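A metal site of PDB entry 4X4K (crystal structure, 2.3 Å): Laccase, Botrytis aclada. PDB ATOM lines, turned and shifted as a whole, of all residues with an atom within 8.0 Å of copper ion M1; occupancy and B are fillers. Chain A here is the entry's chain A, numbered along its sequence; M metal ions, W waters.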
ATOM      1  N   HIS A 124     -15.744  -2.596 -11.701  1.00  0.00           N
ATOM      2  CA  HIS A 124     -14.550  -1.903 -12.127  1.00  0.00           C
ATOM      3  C   HIS A 124     -14.599  -0.395 -11.867  1.00  0.00           C
ATOM      4  O   HIS A 124     -15.619   0.268 -12.028  1.00  0.00           O
ATOM      5  CB  HIS A 124     -14.286  -2.207 -13.603  1.00  0.00           C
ATOM      6  CG  HIS A 124     -13.198  -1.389 -14.198  1.00  0.00           C
ATOM      7  ND1 HIS A 124     -11.886  -1.500 -13.810  1.00  0.00           N
ATOM      8  CD2 HIS A 124     -13.220  -0.447 -15.168  1.00  0.00           C
ATOM      9  CE1 HIS A 124     -11.135  -0.684 -14.521  1.00  0.00           C
ATOM     10  NE2 HIS A 124     -11.931  -0.019 -15.352  1.00  0.00           N
ATOM     11  N   HIS A 126     -13.309   2.777 -13.172  1.00  0.00           N
ATOM     12  CA  HIS A 126     -12.830   3.100 -14.501  1.00  0.00           C
ATOM     13  C   HIS A 126     -11.755   4.157 -14.470  1.00  0.00           C
ATOM     14  O   HIS A 126     -11.954   5.234 -13.934  1.00  0.00           O
ATOM     15  CB  HIS A 126     -13.972   3.544 -15.424  1.00  0.00           C
ATOM     16  CG  HIS A 126     -13.532   3.900 -16.801  1.00  0.00           C
ATOM     17  ND1 HIS A 126     -13.924   3.194 -17.911  1.00  0.00           N
ATOM     18  CD2 HIS A 126     -12.685   4.865 -17.249  1.00  0.00           C
ATOM     19  CE1 HIS A 126     -13.356   3.717 -18.987  1.00  0.00           C
ATOM     20  NE2 HIS A 126     -12.602   4.731 -18.611  1.00  0.00           N
ATOM     21  N   GLY A 127     -10.604   3.814 -15.042  1.00  0.00           N
ATOM     22  CA  GLY A 127      -9.485   4.753 -15.150  1.00  0.00           C
ATOM     23  C   GLY A 127      -8.627   4.785 -13.906  1.00  0.00           C
ATOM     24  O   GLY A 127      -7.570   5.441 -13.895  1.00  0.00           O
ATOM     25  N   ASP A 137      -9.149  -4.440  -9.658  1.00  0.00           N
ATOM     26  CA  ASP A 137      -9.524  -3.724 -10.899  1.00  0.00           C
ATOM     27  C   ASP A 137     -10.922  -4.068 -11.353  1.00  0.00           C
ATOM     28  O   ASP A 137     -11.503  -3.363 -12.184  1.00  0.00           O
ATOM     29  CB  ASP A 137      -8.523  -4.036 -12.016  1.00  0.00           C
ATOM     30  CG  ASP A 137      -8.630  -3.062 -13.194  1.00  0.00           C
ATOM     31  OD1 ASP A 137      -8.739  -1.860 -12.945  1.00  0.00           O
ATOM     32  OD2 ASP A 137      -8.609  -3.506 -14.366  1.00  0.00           O
ATOM     33  N   GLY A 138     -11.476  -5.159 -10.835  1.00  0.00           N
ATOM     34  CA  GLY A 138     -12.846  -5.501 -11.120  1.00  0.00           C
ATOM     35  C   GLY A 138     -13.178  -6.108 -12.464  1.00  0.00           C
ATOM     36  O   GLY A 138     -14.329  -6.082 -12.876  1.00  0.00           O
ATOM     37  N   VAL A 139     -12.194  -6.669 -13.164  1.00  0.00           N
ATOM     38  CA  VAL A 139     -12.468  -7.330 -14.450  1.00  0.00           C
ATOM     39  C   VAL A 139     -12.645  -8.856 -14.279  1.00  0.00           C
ATOM     40  O   VAL A 139     -11.691  -9.549 -13.954  1.00  0.00           O
ATOM     41  CB  VAL A 139     -11.376  -7.025 -15.474  1.00  0.00           C
ATOM     42  CG1 VAL A 139     -11.709  -7.652 -16.807  1.00  0.00           C
ATOM     43  CG2 VAL A 139     -11.233  -5.536 -15.642  1.00  0.00           C
ATOM     44  N   HIS A 168     -18.479   0.827 -12.700  1.00  0.00           N
ATOM     45  CA  HIS A 168     -19.539   0.095 -13.350  1.00  0.00           C
ATOM     46  C   HIS A 168     -19.222  -1.380 -13.281  1.00  0.00           C
ATOM     47  O   HIS A 168     -18.074  -1.762 -13.091  1.00  0.00           O
ATOM     48  CB  HIS A 168     -19.685   0.553 -14.805  1.00  0.00           C
ATOM     49  CG  HIS A 168     -18.432   0.446 -15.637  1.00  0.00           C
ATOM     50  ND1 HIS A 168     -18.003  -0.734 -16.210  1.00  0.00           N
ATOM     51  CD2 HIS A 168     -17.555   1.399 -16.046  1.00  0.00           C
ATOM     52  CE1 HIS A 168     -16.915  -0.511 -16.912  1.00  0.00           C
ATOM     53  NE2 HIS A 168     -16.620   0.779 -16.833  1.00  0.00           N
ATOM     54  N   SER A 169     -20.232  -2.215 -13.450  1.00  0.00           N
ATOM     55  CA  SER A 169     -19.927  -3.632 -13.573  1.00  0.00           C
ATOM     56  C   SER A 169     -19.116  -3.880 -14.823  1.00  0.00           C
ATOM     57  O   SER A 169     -19.294  -3.196 -15.822  1.00  0.00           O
ATOM     58  CB  SER A 169     -21.176  -4.483 -13.641  1.00  0.00           C
ATOM     59  OG  SER A 169     -20.790  -5.737 -14.131  1.00  0.00           O
ATOM     60  N   HIS A 170     -18.242  -4.874 -14.758  1.00  0.00           N
ATOM     61  CA  HIS A 170     -17.483  -5.285 -15.913  1.00  0.00           C
ATOM     62  C   HIS A 170     -17.900  -6.692 -16.265  1.00  0.00           C
ATOM     63  O   HIS A 170     -17.280  -7.334 -17.098  1.00  0.00           O
ATOM     64  CB  HIS A 170     -15.976  -5.188 -15.679  1.00  0.00           C
ATOM     65  CG  HIS A 170     -15.227  -4.624 -16.844  1.00  0.00           C
ATOM     66  ND1 HIS A 170     -15.271  -5.195 -18.101  1.00  0.00           N
ATOM     67  CD2 HIS A 170     -14.455  -3.523 -16.961  1.00  0.00           C
ATOM     68  CE1 HIS A 170     -14.553  -4.469 -18.938  1.00  0.00           C
ATOM     69  NE2 HIS A 170     -14.048  -3.444 -18.271  1.00  0.00           N
ATOM     70  N   TYR A 175     -23.596  -3.157 -16.911  1.00  0.00           N
ATOM     71  CA  TYR A 175     -23.675  -1.681 -16.810  1.00  0.00           C
ATOM     72  C   TYR A 175     -24.741  -1.083 -17.719  1.00  0.00           C
ATOM     73  O   TYR A 175     -25.240   0.015 -17.451  1.00  0.00           O
ATOM     74  CB  TYR A 175     -22.327  -0.975 -16.942  1.00  0.00           C
ATOM     75  CG  TYR A 175     -21.856  -0.602 -18.332  1.00  0.00           C
ATOM     76  CD1 TYR A 175     -22.315   0.550 -18.928  1.00  0.00           C
ATOM     77  CD2 TYR A 175     -20.890  -1.372 -19.007  1.00  0.00           C
ATOM     78  CE1 TYR A 175     -21.878   0.919 -20.176  1.00  0.00           C
ATOM     79  CE2 TYR A 175     -20.434  -1.005 -20.276  1.00  0.00           C
ATOM     80  CZ  TYR A 175     -20.953   0.153 -20.860  1.00  0.00           C
ATOM     81  OH  TYR A 175     -20.562   0.577 -22.117  1.00  0.00           O
ATOM     82  N   HIS A 466     -10.485   1.550 -24.508  1.00  0.00           N
ATOM     83  CA  HIS A 466     -10.177   1.769 -23.115  1.00  0.00           C
ATOM     84  C   HIS A 466      -9.044   0.873 -22.613  1.00  0.00           C
ATOM     85  O   HIS A 466      -9.142  -0.336 -22.722  1.00  0.00           O
ATOM     86  CB  HIS A 466     -11.419   1.554 -22.256  1.00  0.00           C
ATOM     87  CG  HIS A 466     -11.155   1.698 -20.789  1.00  0.00           C
ATOM     88  ND1 HIS A 466     -10.357   2.702 -20.284  1.00  0.00           N
ATOM     89  CD2 HIS A 466     -11.526   0.936 -19.735  1.00  0.00           C
ATOM     90  CE1 HIS A 466     -10.267   2.567 -18.973  1.00  0.00           C
ATOM     91  NE2 HIS A 466     -10.975   1.506 -18.620  1.00  0.00           N
ATOM     92  N   LEU A 467      -7.991   1.482 -22.080  1.00  0.00           N
ATOM     93  CA  LEU A 467      -6.896   0.755 -21.420  1.00  0.00           C
ATOM     94  C   LEU A 467      -6.986   0.752 -19.894  1.00  0.00           C
ATOM     95  O   LEU A 467      -7.071   1.821 -19.263  1.00  0.00           O
ATOM     96  CB  LEU A 467      -5.533   1.321 -21.830  1.00  0.00           C
ATOM     97  CG  LEU A 467      -4.293   0.650 -21.178  1.00  0.00           C
ATOM     98  CD1 LEU A 467      -4.184  -0.816 -21.561  1.00  0.00           C
ATOM     99  CD2 LEU A 467      -2.998   1.407 -21.479  1.00  0.00           C
ATOM    100  N   HIS A 468      -6.952  -0.431 -19.299  1.00  0.00           N
ATOM    101  CA  HIS A 468      -6.887  -0.580 -17.837  1.00  0.00           C
ATOM    102  C   HIS A 468      -5.464  -0.428 -17.320  1.00  0.00           C
ATOM    103  O   HIS A 468      -4.493  -0.687 -18.057  1.00  0.00           O
ATOM    104  CB  HIS A 468      -7.418  -1.937 -17.404  1.00  0.00           C
ATOM    105  CG  HIS A 468      -8.898  -2.095 -17.578  1.00  0.00           C
ATOM    106  ND1 HIS A 468      -9.724  -2.545 -16.573  1.00  0.00           N
ATOM    107  CD2 HIS A 468      -9.697  -1.898 -18.650  1.00  0.00           C
ATOM    108  CE1 HIS A 468     -10.972  -2.591 -16.999  1.00  0.00           C
ATOM    109  NE2 HIS A 468     -10.988  -2.220 -18.258  1.00  0.00           N
ATOM    110  N   VAL A 501      -9.541   6.593 -22.306  1.00  0.00           N
ATOM    111  CA  VAL A 501     -10.398   6.201 -23.432  1.00  0.00           C
ATOM    112  C   VAL A 501     -10.110   7.099 -24.615  1.00  0.00           C
ATOM    113  O   VAL A 501     -10.111   8.318 -24.471  1.00  0.00           O
ATOM    114  CB  VAL A 501     -11.899   6.238 -23.099  1.00  0.00           C
ATOM    115  CG1 VAL A 501     -12.731   5.813 -24.296  1.00  0.00           C
ATOM    116  CG2 VAL A 501     -12.190   5.311 -21.935  1.00  0.00           C
ATOM    117  N   LEU A 523      -6.659  -5.316 -19.125  1.00  0.00           N
ATOM    118  CA  LEU A 523      -7.559  -5.423 -20.266  1.00  0.00           C
ATOM    119  C   LEU A 523      -7.500  -4.123 -21.058  1.00  0.00           C
ATOM    120  O   LEU A 523      -7.335  -3.048 -20.477  1.00  0.00           O
ATOM    121  CB  LEU A 523      -8.979  -5.660 -19.780  1.00  0.00           C
ATOM    122  CG  LEU A 523     -10.079  -5.897 -20.829  1.00  0.00           C
ATOM    123  CD1 LEU A 523      -9.870  -7.239 -21.490  1.00  0.00           C
ATOM    124  CD2 LEU A 523     -11.446  -5.864 -20.161  1.00  0.00           C
ATOM    125  N   LEU A 524      -7.585  -4.249 -22.383  1.00  0.00           N
ATOM    126  CA  LEU A 524      -7.787  -3.128 -23.260  1.00  0.00           C
ATOM    127  C   LEU A 524      -8.933  -3.607 -24.132  1.00  0.00           C
ATOM    128  O   LEU A 524      -8.939  -4.763 -24.587  1.00  0.00           O
ATOM    129  CB  LEU A 524      -6.551  -2.882 -24.098  1.00  0.00           C
ATOM    130  CG  LEU A 524      -6.734  -1.870 -25.234  1.00  0.00           C
ATOM    131  CD1 LEU A 524      -5.502  -1.003 -25.375  1.00  0.00           C
ATOM    132  CD2 LEU A 524      -7.062  -2.547 -26.567  1.00  0.00           C
ATOM    133  N   HIS A 525      -9.916  -2.738 -24.359  1.00  0.00           N
ATOM    134  CA  HIS A 525     -11.100  -3.168 -25.050  1.00  0.00           C
ATOM    135  C   HIS A 525     -11.870  -2.017 -25.633  1.00  0.00           C
ATOM    136  O   HIS A 525     -11.704  -0.847 -25.225  1.00  0.00           O
ATOM    137  CB  HIS A 525     -11.994  -3.996 -24.113  1.00  0.00           C
ATOM    138  CG  HIS A 525     -12.507  -3.225 -22.937  1.00  0.00           C
ATOM    139  ND1 HIS A 525     -13.759  -2.636 -22.927  1.00  0.00           N
ATOM    140  CD2 HIS A 525     -11.927  -2.907 -21.757  1.00  0.00           C
ATOM    141  CE1 HIS A 525     -13.924  -1.999 -21.772  1.00  0.00           C
ATOM    142  NE2 HIS A 525     -12.833  -2.152 -21.054  1.00  0.00           N
ATOM    143  N   CYS A 526     -12.723  -2.335 -26.611  1.00  0.00           N
ATOM    144  CA  CYS A 526     -13.685  -1.363 -27.042  1.00  0.00           C
ATOM    145  C   CYS A 526     -14.681  -1.221 -25.892  1.00  0.00           C
ATOM    146  O   CYS A 526     -15.094  -2.242 -25.301  1.00  0.00           O
ATOM    147  CB  CYS A 526     -14.400  -1.801 -28.304  1.00  0.00           C
ATOM    148  SG  CYS A 526     -15.592  -0.559 -28.841  1.00  0.00           S
ATOM    149  N   HIS A 527     -15.033   0.026 -25.573  1.00  0.00           N
ATOM    150  CA  HIS A 527     -16.001   0.293 -24.517  1.00  0.00           C
ATOM    151  C   HIS A 527     -17.457   0.286 -24.966  1.00  0.00           C
ATOM    152  O   HIS A 527     -18.368   0.512 -24.151  1.00  0.00           O
ATOM    153  CB  HIS A 527     -15.669   1.588 -23.768  1.00  0.00           C
ATOM    154  CG  HIS A 527     -15.908   1.497 -22.285  1.00  0.00           C
ATOM    155  ND1 HIS A 527     -17.141   1.194 -21.745  1.00  0.00           N
ATOM    156  CD2 HIS A 527     -15.065   1.677 -21.233  1.00  0.00           C
ATOM    157  CE1 HIS A 527     -17.049   1.179 -20.427  1.00  0.00           C
ATOM    158  NE2 HIS A 527     -15.811   1.485 -20.086  1.00  0.00           N
ATOM    159  N   ALA A 532     -17.413  -5.257 -26.679  1.00  0.00           N
ATOM    160  CA  ALA A 532     -16.672  -5.861 -25.596  1.00  0.00           C
ATOM    161  C   ALA A 532     -17.162  -7.298 -25.434  1.00  0.00           C
ATOM    162  O   ALA A 532     -16.365  -8.226 -25.457  1.00  0.00           O
ATOM    163  CB  ALA A 532     -16.887  -5.065 -24.323  1.00  0.00           C
ATOM    164  N   ILE A 580     -16.359 -10.218 -20.458  1.00  0.00           N
ATOM    165  CA  ILE A 580     -16.163  -8.848 -20.006  1.00  0.00           C
ATOM    166  C   ILE A 580     -17.241  -7.908 -20.511  1.00  0.00           C
ATOM    167  O   ILE A 580     -18.269  -8.349 -21.059  1.00  0.00           O
ATOM    168  CB  ILE A 580     -14.788  -8.282 -20.387  1.00  0.00           C
ATOM    169  CG1 ILE A 580     -14.552  -8.443 -21.885  1.00  0.00           C
ATOM    170  CG2 ILE A 580     -13.704  -8.965 -19.587  1.00  0.00           C
ATOM    171  CD1 ILE A 580     -13.963  -7.239 -22.547  1.00  0.00           C
ATOM    172  OXT ILE A 580     -17.092  -6.692 -20.384  1.00  0.00           O
HETATM  173 CU    CU M   1     -12.724  -2.132 -19.137  1.00  0.00          CU
HETATM  174 CU    CU M   2     -11.382   0.780 -17.055  1.00  0.00          CU
HETATM  175 CU    CU M   3     -15.325   1.713 -18.059  1.00  0.00          CU
HETATM  176  O   HOH W   1     -13.959  -0.572 -18.758  1.00  0.00           O
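Copper ion M1 is bound by NE2 of His 525 (1.9 Å), NE2 of His 468 (1.9 Å), water W1 (2.0 Å) and NE2 of His 170 (2.1 Å). Copper ion M1 has four donor atoms within binding distance.
Merely in contact with copper ion M1: His 466. Of the 21 residues printed, 4 come within 4 Å of copper ion M1. Along chain A the residues within 4 Å of copper ion M1 span positions 170 to 525.
O of His 525 is in hydrogen-bond range of N of His 466 (2.8 Å). The backbone NH of His 468 sits at hydrogen-bond distance from the backbone carbonyl oxygen of Leu 523, at 2.9 Å. ND1 of His 468 is in hydrogen-bond range of OD2 of Asp 137, 2.7 Å away. A ring nitrogen (ND1) of His 170 lies within hydrogen-bond range of the chain-end carboxylate (OXT) of Ile 580. ND1 of His 466 sits close to NE2 of His 126 (3.5 Å).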
